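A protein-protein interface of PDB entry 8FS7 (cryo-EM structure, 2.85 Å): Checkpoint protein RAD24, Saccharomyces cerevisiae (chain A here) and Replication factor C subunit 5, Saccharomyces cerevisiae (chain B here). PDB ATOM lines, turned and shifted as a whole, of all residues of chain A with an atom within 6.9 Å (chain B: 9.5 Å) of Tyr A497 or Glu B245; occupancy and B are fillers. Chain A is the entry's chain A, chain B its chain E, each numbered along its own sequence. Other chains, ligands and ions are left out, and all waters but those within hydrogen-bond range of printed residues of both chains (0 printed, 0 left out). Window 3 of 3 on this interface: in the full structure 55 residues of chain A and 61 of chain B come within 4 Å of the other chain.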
ATOM      1  N   ARG A 492     -32.681  32.490  -9.944  1.00  0.00           N
ATOM      2  CA  ARG A 492     -33.154  33.455  -8.955  1.00  0.00           C
ATOM      3  C   ARG A 492     -33.964  32.800  -7.842  1.00  0.00           C
ATOM      4  O   ARG A 492     -34.083  33.381  -6.759  1.00  0.00           O
ATOM      5  CB  ARG A 492     -33.995  34.545  -9.623  1.00  0.00           C
ATOM      6  CG  ARG A 492     -33.291  35.327 -10.727  1.00  0.00           C
ATOM      7  CD  ARG A 492     -31.844  35.646 -10.385  1.00  0.00           C
ATOM      8  NE  ARG A 492     -31.304  36.686 -11.253  1.00  0.00           N
ATOM      9  CZ  ARG A 492     -30.058  37.136 -11.200  1.00  0.00           C
ATOM     10  NH1 ARG A 492     -29.180  36.642 -10.343  1.00  0.00           N
ATOM     11  NH2 ARG A 492     -29.683  38.105 -12.030  1.00  0.00           N
ATOM     12  N   LYS A 493     -34.541  31.628  -8.130  1.00  0.00           N
ATOM     13  CA  LYS A 493     -35.354  30.897  -7.121  1.00  0.00           C
ATOM     14  C   LYS A 493     -34.427  30.362  -6.028  1.00  0.00           C
ATOM     15  O   LYS A 493     -34.536  30.827  -4.877  1.00  0.00           O
ATOM     16  CB  LYS A 493     -36.099  29.732  -7.777  1.00  0.00           C
ATOM     17  CG  LYS A 493     -37.591  29.941  -7.991  1.00  0.00           C
ATOM     18  CD  LYS A 493     -38.370  30.018  -6.696  1.00  0.00           C
ATOM     19  CE  LYS A 493     -39.851  30.246  -6.912  1.00  0.00           C
ATOM     20  NZ  LYS A 493     -40.458  29.165  -7.722  1.00  0.00           N
ATOM     21  N   CYS A 494     -33.550  29.424  -6.389  1.00  0.00           N
ATOM     22  CA  CYS A 494     -32.631  28.820  -5.390  1.00  0.00           C
ATOM     23  C   CYS A 494     -31.804  29.928  -4.733  1.00  0.00           C
ATOM     24  O   CYS A 494     -31.719  29.943  -3.495  1.00  0.00           O
ATOM     25  CB  CYS A 494     -31.714  27.800  -6.048  1.00  0.00           C
ATOM     26  SG  CYS A 494     -32.598  26.336  -6.644  1.00  0.00           S
ATOM     27  N   GLN A 495     -31.255  30.840  -5.538  1.00  0.00           N
ATOM     28  CA  GLN A 495     -30.427  31.946  -4.989  1.00  0.00           C
ATOM     29  C   GLN A 495     -31.212  32.635  -3.868  1.00  0.00           C
ATOM     30  O   GLN A 495     -30.613  32.905  -2.811  1.00  0.00           O
ATOM     31  CB  GLN A 495     -30.067  32.940  -6.093  1.00  0.00           C
ATOM     32  CG  GLN A 495     -29.081  34.014  -5.662  1.00  0.00           C
ATOM     33  CD  GLN A 495     -28.831  35.010  -6.767  1.00  0.00           C
ATOM     34  OE1 GLN A 495     -28.407  34.657  -7.864  1.00  0.00           O
ATOM     35  NE2 GLN A 495     -29.105  36.274  -6.485  1.00  0.00           N
ATOM     36  N   SER A 496     -32.502  32.901  -4.095  1.00  0.00           N
ATOM     37  CA  SER A 496     -33.325  33.654  -3.113  1.00  0.00           C
ATOM     38  C   SER A 496     -33.719  32.762  -1.930  1.00  0.00           C
ATOM     39  O   SER A 496     -33.509  33.192  -0.781  1.00  0.00           O
ATOM     40  CB  SER A 496     -34.542  34.249  -3.772  1.00  0.00           C
ATOM     41  OG  SER A 496     -35.343  34.937  -2.822  1.00  0.00           O
ATOM     42  N   TYR A 497     -34.270  31.572  -2.195  1.00  0.00           N
ATOM     43  CA  TYR A 497     -34.762  30.712  -1.084  1.00  0.00           C
ATOM     44  C   TYR A 497     -33.577  30.241  -0.230  1.00  0.00           C
ATOM     45  O   TYR A 497     -33.706  30.220   1.009  1.00  0.00           O
ATOM     46  CB  TYR A 497     -35.621  29.555  -1.612  1.00  0.00           C
ATOM     47  CG  TYR A 497     -34.962  28.199  -1.629  1.00  0.00           C
ATOM     48  CD1 TYR A 497     -33.983  27.887  -2.556  1.00  0.00           C
ATOM     49  CD2 TYR A 497     -35.310  27.225  -0.707  1.00  0.00           C
ATOM     50  CE1 TYR A 497     -33.369  26.645  -2.573  1.00  0.00           C
ATOM     51  CE2 TYR A 497     -34.707  25.978  -0.709  1.00  0.00           C
ATOM     52  CZ  TYR A 497     -33.732  25.686  -1.646  1.00  0.00           C
ATOM     53  OH  TYR A 497     -33.129  24.452  -1.658  1.00  0.00           O
ATOM     54  N   LYS A 498     -32.462  29.880  -0.872  1.00  0.00           N
ATOM     55  CA  LYS A 498     -31.273  29.390  -0.125  1.00  0.00           C
ATOM     56  C   LYS A 498     -30.714  30.546   0.709  1.00  0.00           C
ATOM     57  O   LYS A 498     -30.291  30.295   1.852  1.00  0.00           O
ATOM     58  CB  LYS A 498     -30.226  28.823  -1.089  1.00  0.00           C
ATOM     59  CG  LYS A 498     -29.124  27.999  -0.437  1.00  0.00           C
ATOM     60  CD  LYS A 498     -28.227  27.314  -1.444  1.00  0.00           C
ATOM     61  CE  LYS A 498     -28.993  26.450  -2.423  1.00  0.00           C
ATOM     62  NZ  LYS A 498     -28.080  25.686  -3.306  1.00  0.00           N
ATOM     63  N   LYS A 499     -30.723  31.762   0.155  1.00  0.00           N
ATOM     64  CA  LYS A 499     -30.254  32.953   0.913  1.00  0.00           C
ATOM     65  C   LYS A 499     -31.015  33.028   2.242  1.00  0.00           C
ATOM     66  O   LYS A 499     -32.261  33.030   2.186  1.00  0.00           O
ATOM     67  CB  LYS A 499     -30.470  34.226   0.092  1.00  0.00           C
ATOM     68  CG  LYS A 499     -30.192  35.529   0.829  1.00  0.00           C
ATOM     69  CD  LYS A 499     -30.526  36.759   0.014  1.00  0.00           C
ATOM     70  CE  LYS A 499     -30.277  38.050   0.763  1.00  0.00           C
ATOM     71  NZ  LYS A 499     -30.616  39.235  -0.060  1.00  0.00           N
ATOM     72  N   VAL A 536     -38.592  36.084 -10.235  1.00  0.00           N
ATOM     73  CA  VAL A 536     -38.413  34.715  -9.772  1.00  0.00           C
ATOM     74  C   VAL A 536     -39.263  33.712 -10.540  1.00  0.00           C
ATOM     75  O   VAL A 536     -38.897  32.526 -10.592  1.00  0.00           O
ATOM     76  CB  VAL A 536     -38.698  34.600  -8.258  1.00  0.00           C
ATOM     77  CG1 VAL A 536     -37.914  33.449  -7.652  1.00  0.00           C
ATOM     78  CG2 VAL A 536     -38.374  35.906  -7.545  1.00  0.00           C
ATOM     79  N   GLU B 209     -15.037  28.651  -8.162  1.00  0.00           N
ATOM     80  CA  GLU B 209     -16.012  28.474  -7.086  1.00  0.00           C
ATOM     81  C   GLU B 209     -16.233  26.979  -6.901  1.00  0.00           C
ATOM     82  O   GLU B 209     -16.820  26.328  -7.771  1.00  0.00           O
ATOM     83  CB  GLU B 209     -17.322  29.197  -7.399  1.00  0.00           C
ATOM     84  CG  GLU B 209     -18.517  28.709  -6.589  1.00  0.00           C
ATOM     85  CD  GLU B 209     -19.698  29.659  -6.657  1.00  0.00           C
ATOM     86  OE1 GLU B 209     -19.642  30.624  -7.448  1.00  0.00           O
ATOM     87  OE2 GLU B 209     -20.680  29.441  -5.918  1.00  0.00           O
ATOM     88  N   ARG B 210     -15.763  26.443  -5.773  1.00  0.00           N
ATOM     89  CA  ARG B 210     -15.803  25.003  -5.542  1.00  0.00           C
ATOM     90  C   ARG B 210     -17.238  24.495  -5.476  1.00  0.00           C
ATOM     91  O   ARG B 210     -18.092  25.087  -4.809  1.00  0.00           O
ATOM     92  CB  ARG B 210     -15.059  24.658  -4.251  1.00  0.00           C
ATOM     93  CG  ARG B 210     -14.280  23.351  -4.310  1.00  0.00           C
ATOM     94  CD  ARG B 210     -13.399  23.269  -5.550  1.00  0.00           C
ATOM     95  NE  ARG B 210     -12.525  24.429  -5.687  1.00  0.00           N
ATOM     96  CZ  ARG B 210     -11.319  24.525  -5.143  1.00  0.00           C
ATOM     97  NH1 ARG B 210     -10.808  23.546  -4.416  1.00  0.00           N
ATOM     98  NH2 ARG B 210     -10.608  25.633  -5.334  1.00  0.00           N
ATOM     99  N   ILE B 211     -17.499  23.392  -6.176  1.00  0.00           N
ATOM    100  CA  ILE B 211     -18.847  22.849  -6.302  1.00  0.00           C
ATOM    101  C   ILE B 211     -18.840  21.351  -5.999  1.00  0.00           C
ATOM    102  O   ILE B 211     -19.763  20.621  -6.385  1.00  0.00           O
ATOM    103  CB  ILE B 211     -19.418  23.168  -7.700  1.00  0.00           C
ATOM    104  CG1 ILE B 211     -20.947  23.227  -7.661  1.00  0.00           C
ATOM    105  CG2 ILE B 211     -18.867  22.223  -8.775  1.00  0.00           C
ATOM    106  CD1 ILE B 211     -21.476  24.110  -6.557  1.00  0.00           C
ATOM    107  N   GLN B 212     -17.810  20.902  -5.270  1.00  0.00           N
ATOM    108  CA  GLN B 212     -17.542  19.502  -4.941  1.00  0.00           C
ATOM    109  C   GLN B 212     -17.090  18.739  -6.183  1.00  0.00           C
ATOM    110  O   GLN B 212     -15.940  18.290  -6.241  1.00  0.00           O
ATOM    111  CB  GLN B 212     -18.755  18.827  -4.282  1.00  0.00           C
ATOM    112  CG  GLN B 212     -18.722  17.302  -4.278  1.00  0.00           C
ATOM    113  CD  GLN B 212     -17.613  16.738  -3.413  1.00  0.00           C
ATOM    114  OE1 GLN B 212     -17.175  17.370  -2.452  1.00  0.00           O
ATOM    115  NE2 GLN B 212     -17.155  15.537  -3.750  1.00  0.00           N
ATOM    116  N   LEU B 237     -24.985  24.236 -15.500  1.00  0.00           N
ATOM    117  CA  LEU B 237     -24.093  24.050 -14.360  1.00  0.00           C
ATOM    118  C   LEU B 237     -24.581  24.837 -13.152  1.00  0.00           C
ATOM    119  O   LEU B 237     -24.623  24.314 -12.033  1.00  0.00           O
ATOM    120  CB  LEU B 237     -22.670  24.464 -14.735  1.00  0.00           C
ATOM    121  CG  LEU B 237     -21.594  24.201 -13.680  1.00  0.00           C
ATOM    122  CD1 LEU B 237     -21.412  22.708 -13.456  1.00  0.00           C
ATOM    123  CD2 LEU B 237     -20.278  24.854 -14.074  1.00  0.00           C
ATOM    124  N   GLU B 238     -24.976  26.095 -13.366  1.00  0.00           N
ATOM    125  CA  GLU B 238     -25.482  26.908 -12.264  1.00  0.00           C
ATOM    126  C   GLU B 238     -26.780  26.338 -11.703  1.00  0.00           C
ATOM    127  O   GLU B 238     -26.988  26.338 -10.485  1.00  0.00           O
ATOM    128  CB  GLU B 238     -25.682  28.352 -12.723  1.00  0.00           C
ATOM    129  CG  GLU B 238     -25.733  29.360 -11.585  1.00  0.00           C
ATOM    130  CD  GLU B 238     -25.495  30.781 -12.053  1.00  0.00           C
ATOM    131  OE1 GLU B 238     -25.108  30.966 -13.226  1.00  0.00           O
ATOM    132  OE2 GLU B 238     -25.696  31.715 -11.248  1.00  0.00           O
ATOM    133  N   SER B 239     -27.662  25.842 -12.576  1.00  0.00           N
ATOM    134  CA  SER B 239     -28.931  25.287 -12.116  1.00  0.00           C
ATOM    135  C   SER B 239     -28.713  24.047 -11.256  1.00  0.00           C
ATOM    136  O   SER B 239     -29.300  23.921 -10.175  1.00  0.00           O
ATOM    137  CB  SER B 239     -29.825  24.965 -13.313  1.00  0.00           C
ATOM    138  OG  SER B 239     -30.014  26.108 -14.130  1.00  0.00           O
ATOM    139  N   MET B 240     -27.865  23.123 -11.718  1.00  0.00           N
ATOM    140  CA  MET B 240     -27.576  21.935 -10.917  1.00  0.00           C
ATOM    141  C   MET B 240     -26.863  22.301  -9.621  1.00  0.00           C
ATOM    142  O   MET B 240     -27.128  21.703  -8.571  1.00  0.00           O
ATOM    143  CB  MET B 240     -26.747  20.926 -11.712  1.00  0.00           C
ATOM    144  CG  MET B 240     -27.279  20.621 -13.097  1.00  0.00           C
ATOM    145  SD  MET B 240     -26.311  19.360 -13.942  1.00  0.00           S
ATOM    146  CE  MET B 240     -27.390  18.986 -15.318  1.00  0.00           C
ATOM    147  N   ALA B 241     -25.956  23.280  -9.673  1.00  0.00           N
ATOM    148  CA  ALA B 241     -25.245  23.697  -8.471  1.00  0.00           C
ATOM    149  C   ALA B 241     -26.199  24.264  -7.428  1.00  0.00           C
ATOM    150  O   ALA B 241     -26.081  23.955  -6.236  1.00  0.00           O
ATOM    151  CB  ALA B 241     -24.176  24.726  -8.834  1.00  0.00           C
ATOM    152  N   LEU B 242     -27.153  25.092  -7.855  1.00  0.00           N
ATOM    153  CA  LEU B 242     -28.064  25.709  -6.898  1.00  0.00           C
ATOM    154  C   LEU B 242     -29.125  24.724  -6.419  1.00  0.00           C
ATOM    155  O   LEU B 242     -29.568  24.796  -5.267  1.00  0.00           O
ATOM    156  CB  LEU B 242     -28.710  26.952  -7.509  1.00  0.00           C
ATOM    157  CG  LEU B 242     -27.998  28.285  -7.244  1.00  0.00           C
ATOM    158  CD1 LEU B 242     -27.814  28.512  -5.750  1.00  0.00           C
ATOM    159  CD2 LEU B 242     -26.660  28.366  -7.965  1.00  0.00           C
ATOM    160  N   ASN B 243     -29.548  23.796  -7.283  1.00  0.00           N
ATOM    161  CA  ASN B 243     -30.567  22.831  -6.884  1.00  0.00           C
ATOM    162  C   ASN B 243     -30.009  21.727  -5.995  1.00  0.00           C
ATOM    163  O   ASN B 243     -30.725  21.224  -5.122  1.00  0.00           O
ATOM    164  CB  ASN B 243     -31.229  22.224  -8.121  1.00  0.00           C
ATOM    165  CG  ASN B 243     -32.053  23.232  -8.897  1.00  0.00           C
ATOM    166  OD1 ASN B 243     -32.088  24.415  -8.557  1.00  0.00           O
ATOM    167  ND2 ASN B 243     -32.724  22.769  -9.945  1.00  0.00           N
ATOM    168  N   ASN B 244     -28.748  21.335  -6.192  1.00  0.00           N
ATOM    169  CA  ASN B 244     -28.140  20.250  -5.431  1.00  0.00           C
ATOM    170  C   ASN B 244     -27.422  20.739  -4.177  1.00  0.00           C
ATOM    171  O   ASN B 244     -26.485  20.077  -3.710  1.00  0.00           O
ATOM    172  CB  ASN B 244     -27.180  19.459  -6.320  1.00  0.00           C
ATOM    173  CG  ASN B 244     -27.886  18.769  -7.473  1.00  0.00           C
ATOM    174  OD1 ASN B 244     -27.270  18.441  -8.487  1.00  0.00           O
ATOM    175  ND2 ASN B 244     -29.186  18.539  -7.320  1.00  0.00           N
ATOM    176  N   GLU B 245     -27.842  21.883  -3.628  1.00  0.00           N
ATOM    177  CA  GLU B 245     -27.308  22.426  -2.376  1.00  0.00           C
ATOM    178  C   GLU B 245     -25.801  22.668  -2.464  1.00  0.00           C
ATOM    179  O   GLU B 245     -25.019  22.160  -1.658  1.00  0.00           O
ATOM    180  CB  GLU B 245     -27.650  21.515  -1.189  1.00  0.00           C
ATOM    181  CG  GLU B 245     -29.149  21.309  -0.900  1.00  0.00           C
ATOM    182  CD  GLU B 245     -29.950  22.585  -0.620  1.00  0.00           C
ATOM    183  OE1 GLU B 245     -29.387  23.702  -0.600  1.00  0.00           O
ATOM    184  OE2 GLU B 245     -31.175  22.462  -0.418  1.00  0.00           O
ATOM    185  N   LEU B 246     -25.402  23.461  -3.463  1.00  0.00           N
ATOM    186  CA  LEU B 246     -24.006  23.849  -3.681  1.00  0.00           C
ATOM    187  C   LEU B 246     -23.093  22.636  -3.844  1.00  0.00           C
ATOM    188  O   LEU B 246     -21.946  22.643  -3.393  1.00  0.00           O
ATOM    189  CB  LEU B 246     -23.497  24.753  -2.552  1.00  0.00           C
ATOM    190  CG  LEU B 246     -23.459  26.257  -2.833  1.00  0.00           C
ATOM    191  CD1 LEU B 246     -22.640  26.561  -4.077  1.00  0.00           C
ATOM    192  CD2 LEU B 246     -24.869  26.817  -2.967  1.00  0.00           C
ATOM    193  N   ALA B 247     -23.595  21.588  -4.494  1.00  0.00           N
ATOM    194  CA  ALA B 247     -22.829  20.373  -4.724  1.00  0.00           C
ATOM    195  C   ALA B 247     -23.230  19.781  -6.067  1.00  0.00           C
ATOM    196  O   ALA B 247     -24.090  20.312  -6.774  1.00  0.00           O
ATOM    197  CB  ALA B 247     -23.036  19.352  -3.598  1.00  0.00           C
ATOM    198  N   LEU B 248     -22.589  18.668  -6.420  1.00  0.00           N
ATOM    199  CA  LEU B 248     -22.879  17.967  -7.662  1.00  0.00           C
ATOM    200  C   LEU B 248     -22.829  16.467  -7.419  1.00  0.00           C
ATOM    201  O   LEU B 248     -22.110  15.987  -6.538  1.00  0.00           O
ATOM    202  CB  LEU B 248     -21.896  18.361  -8.773  1.00  0.00           C
ATOM    203  CG  LEU B 248     -22.175  19.697  -9.468  1.00  0.00           C
ATOM    204  CD1 LEU B 248     -21.179  19.948 -10.587  1.00  0.00           C
ATOM    205  CD2 LEU B 248     -23.600  19.735 -10.000  1.00  0.00           C
ATOM    206  N   LYS B 249     -23.603  15.728  -8.212  1.00  0.00           N
ATOM    207  CA  LYS B 249     -23.719  14.285  -8.078  1.00  0.00           C
ATOM    208  C   LYS B 249     -23.542  13.631  -9.442  1.00  0.00           C
ATOM    209  O   LYS B 249     -23.946  14.183 -10.468  1.00  0.00           O
ATOM    210  CB  LYS B 249     -25.079  13.896  -7.466  1.00  0.00           C
ATOM    211  CG  LYS B 249     -25.333  12.398  -7.351  1.00  0.00           C
ATOM    212  CD  LYS B 249     -24.359  11.745  -6.384  1.00  0.00           C
ATOM    213  CE  LYS B 249     -24.447  10.229  -6.450  1.00  0.00           C
ATOM    214  NZ  LYS B 249     -25.828   9.739  -6.185  1.00  0.00           N
ATOM    215  N   SER B 252     -26.891  13.007 -10.934  1.00  0.00           N
ATOM    216  CA  SER B 252     -27.788  14.151 -10.988  1.00  0.00           C
ATOM    217  C   SER B 252     -28.450  14.232 -12.362  1.00  0.00           C
ATOM    218  O   SER B 252     -27.781  14.042 -13.386  1.00  0.00           O
ATOM    219  CB  SER B 252     -27.029  15.444 -10.691  1.00  0.00           C
ATOM    220  OG  SER B 252     -27.905  16.559 -10.672  1.00  0.00           O
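Of the 18 printed residues of chain B, 5 touch a printed residue of chain A.
Hydrophobic or aromatic side chains of chain B within 4 Å of the printed part of chain A: Leu B242 and Leu B246.
Printed residues of chain A that touch a printed residue of chain B: Cys A494, Tyr A497 and Lys A498.
The backbone carbonyl oxygen (O) of Ser B239 lies close to the side-chain amide oxygen (OD1) of Asn B243 (3.3 Å).
The backbone NH (N) of Leu B246 is in hydrogen-bond range of the backbone carbonyl oxygen (O) of Ala B241, at 2.9 Å.
Among the printed residues, pairs that only touch across the chains: Lys A498 with Ala B241 (3.9 Å).
Tyr A497 touches one residue of chain B.
Glu B245 touches two residues of chain A.
No residue of chain B comes within 4 Å of Ser A496.
Lys A498 touches four residues of chain B.
Of the printed residues of chain A, Leu B246 touches Lys A498 (3.4 Å).
Printed residues of chain A within 4 Å of Ala B241: Lys A498 (3.9 Å).
Printed residues of chain A within 4 Å of Leu B242: Cys A494 and Lys A498.
Printed residues of chain A within 4 Å of Asn B243: Cys A494.
Lys B249 touches none of the printed residues of chain A.
The nearest printed residue of chain A that does not touch Leu B242 is Gln A495 (4.2 Å).
SG of Cys A494 is in hydrogen-bond range of O of Leu B242 (3.7 Å).
The side-chain sulfur (SG) of Cys A494 lies within hydrogen-bond range of the side-chain amide oxygen (OD1) of Asn B243, at 2.8 Å.
The side-chain hydroxyl of Tyr A497 is in hydrogen-bond range of the side-chain carboxylate of Glu B245 (3.1 Å).
NZ of Lys A498 lies within hydrogen-bond range of O of Leu B242, 2.6 Å away.
OE1 of Glu B245 lies within salt-bridge range of NZ of Lys A498, 3.6 Å away.
The side-chain amino group (NZ) of Lys A498 sits close to the backbone NH (N) of Leu B246, 3.5 Å away.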
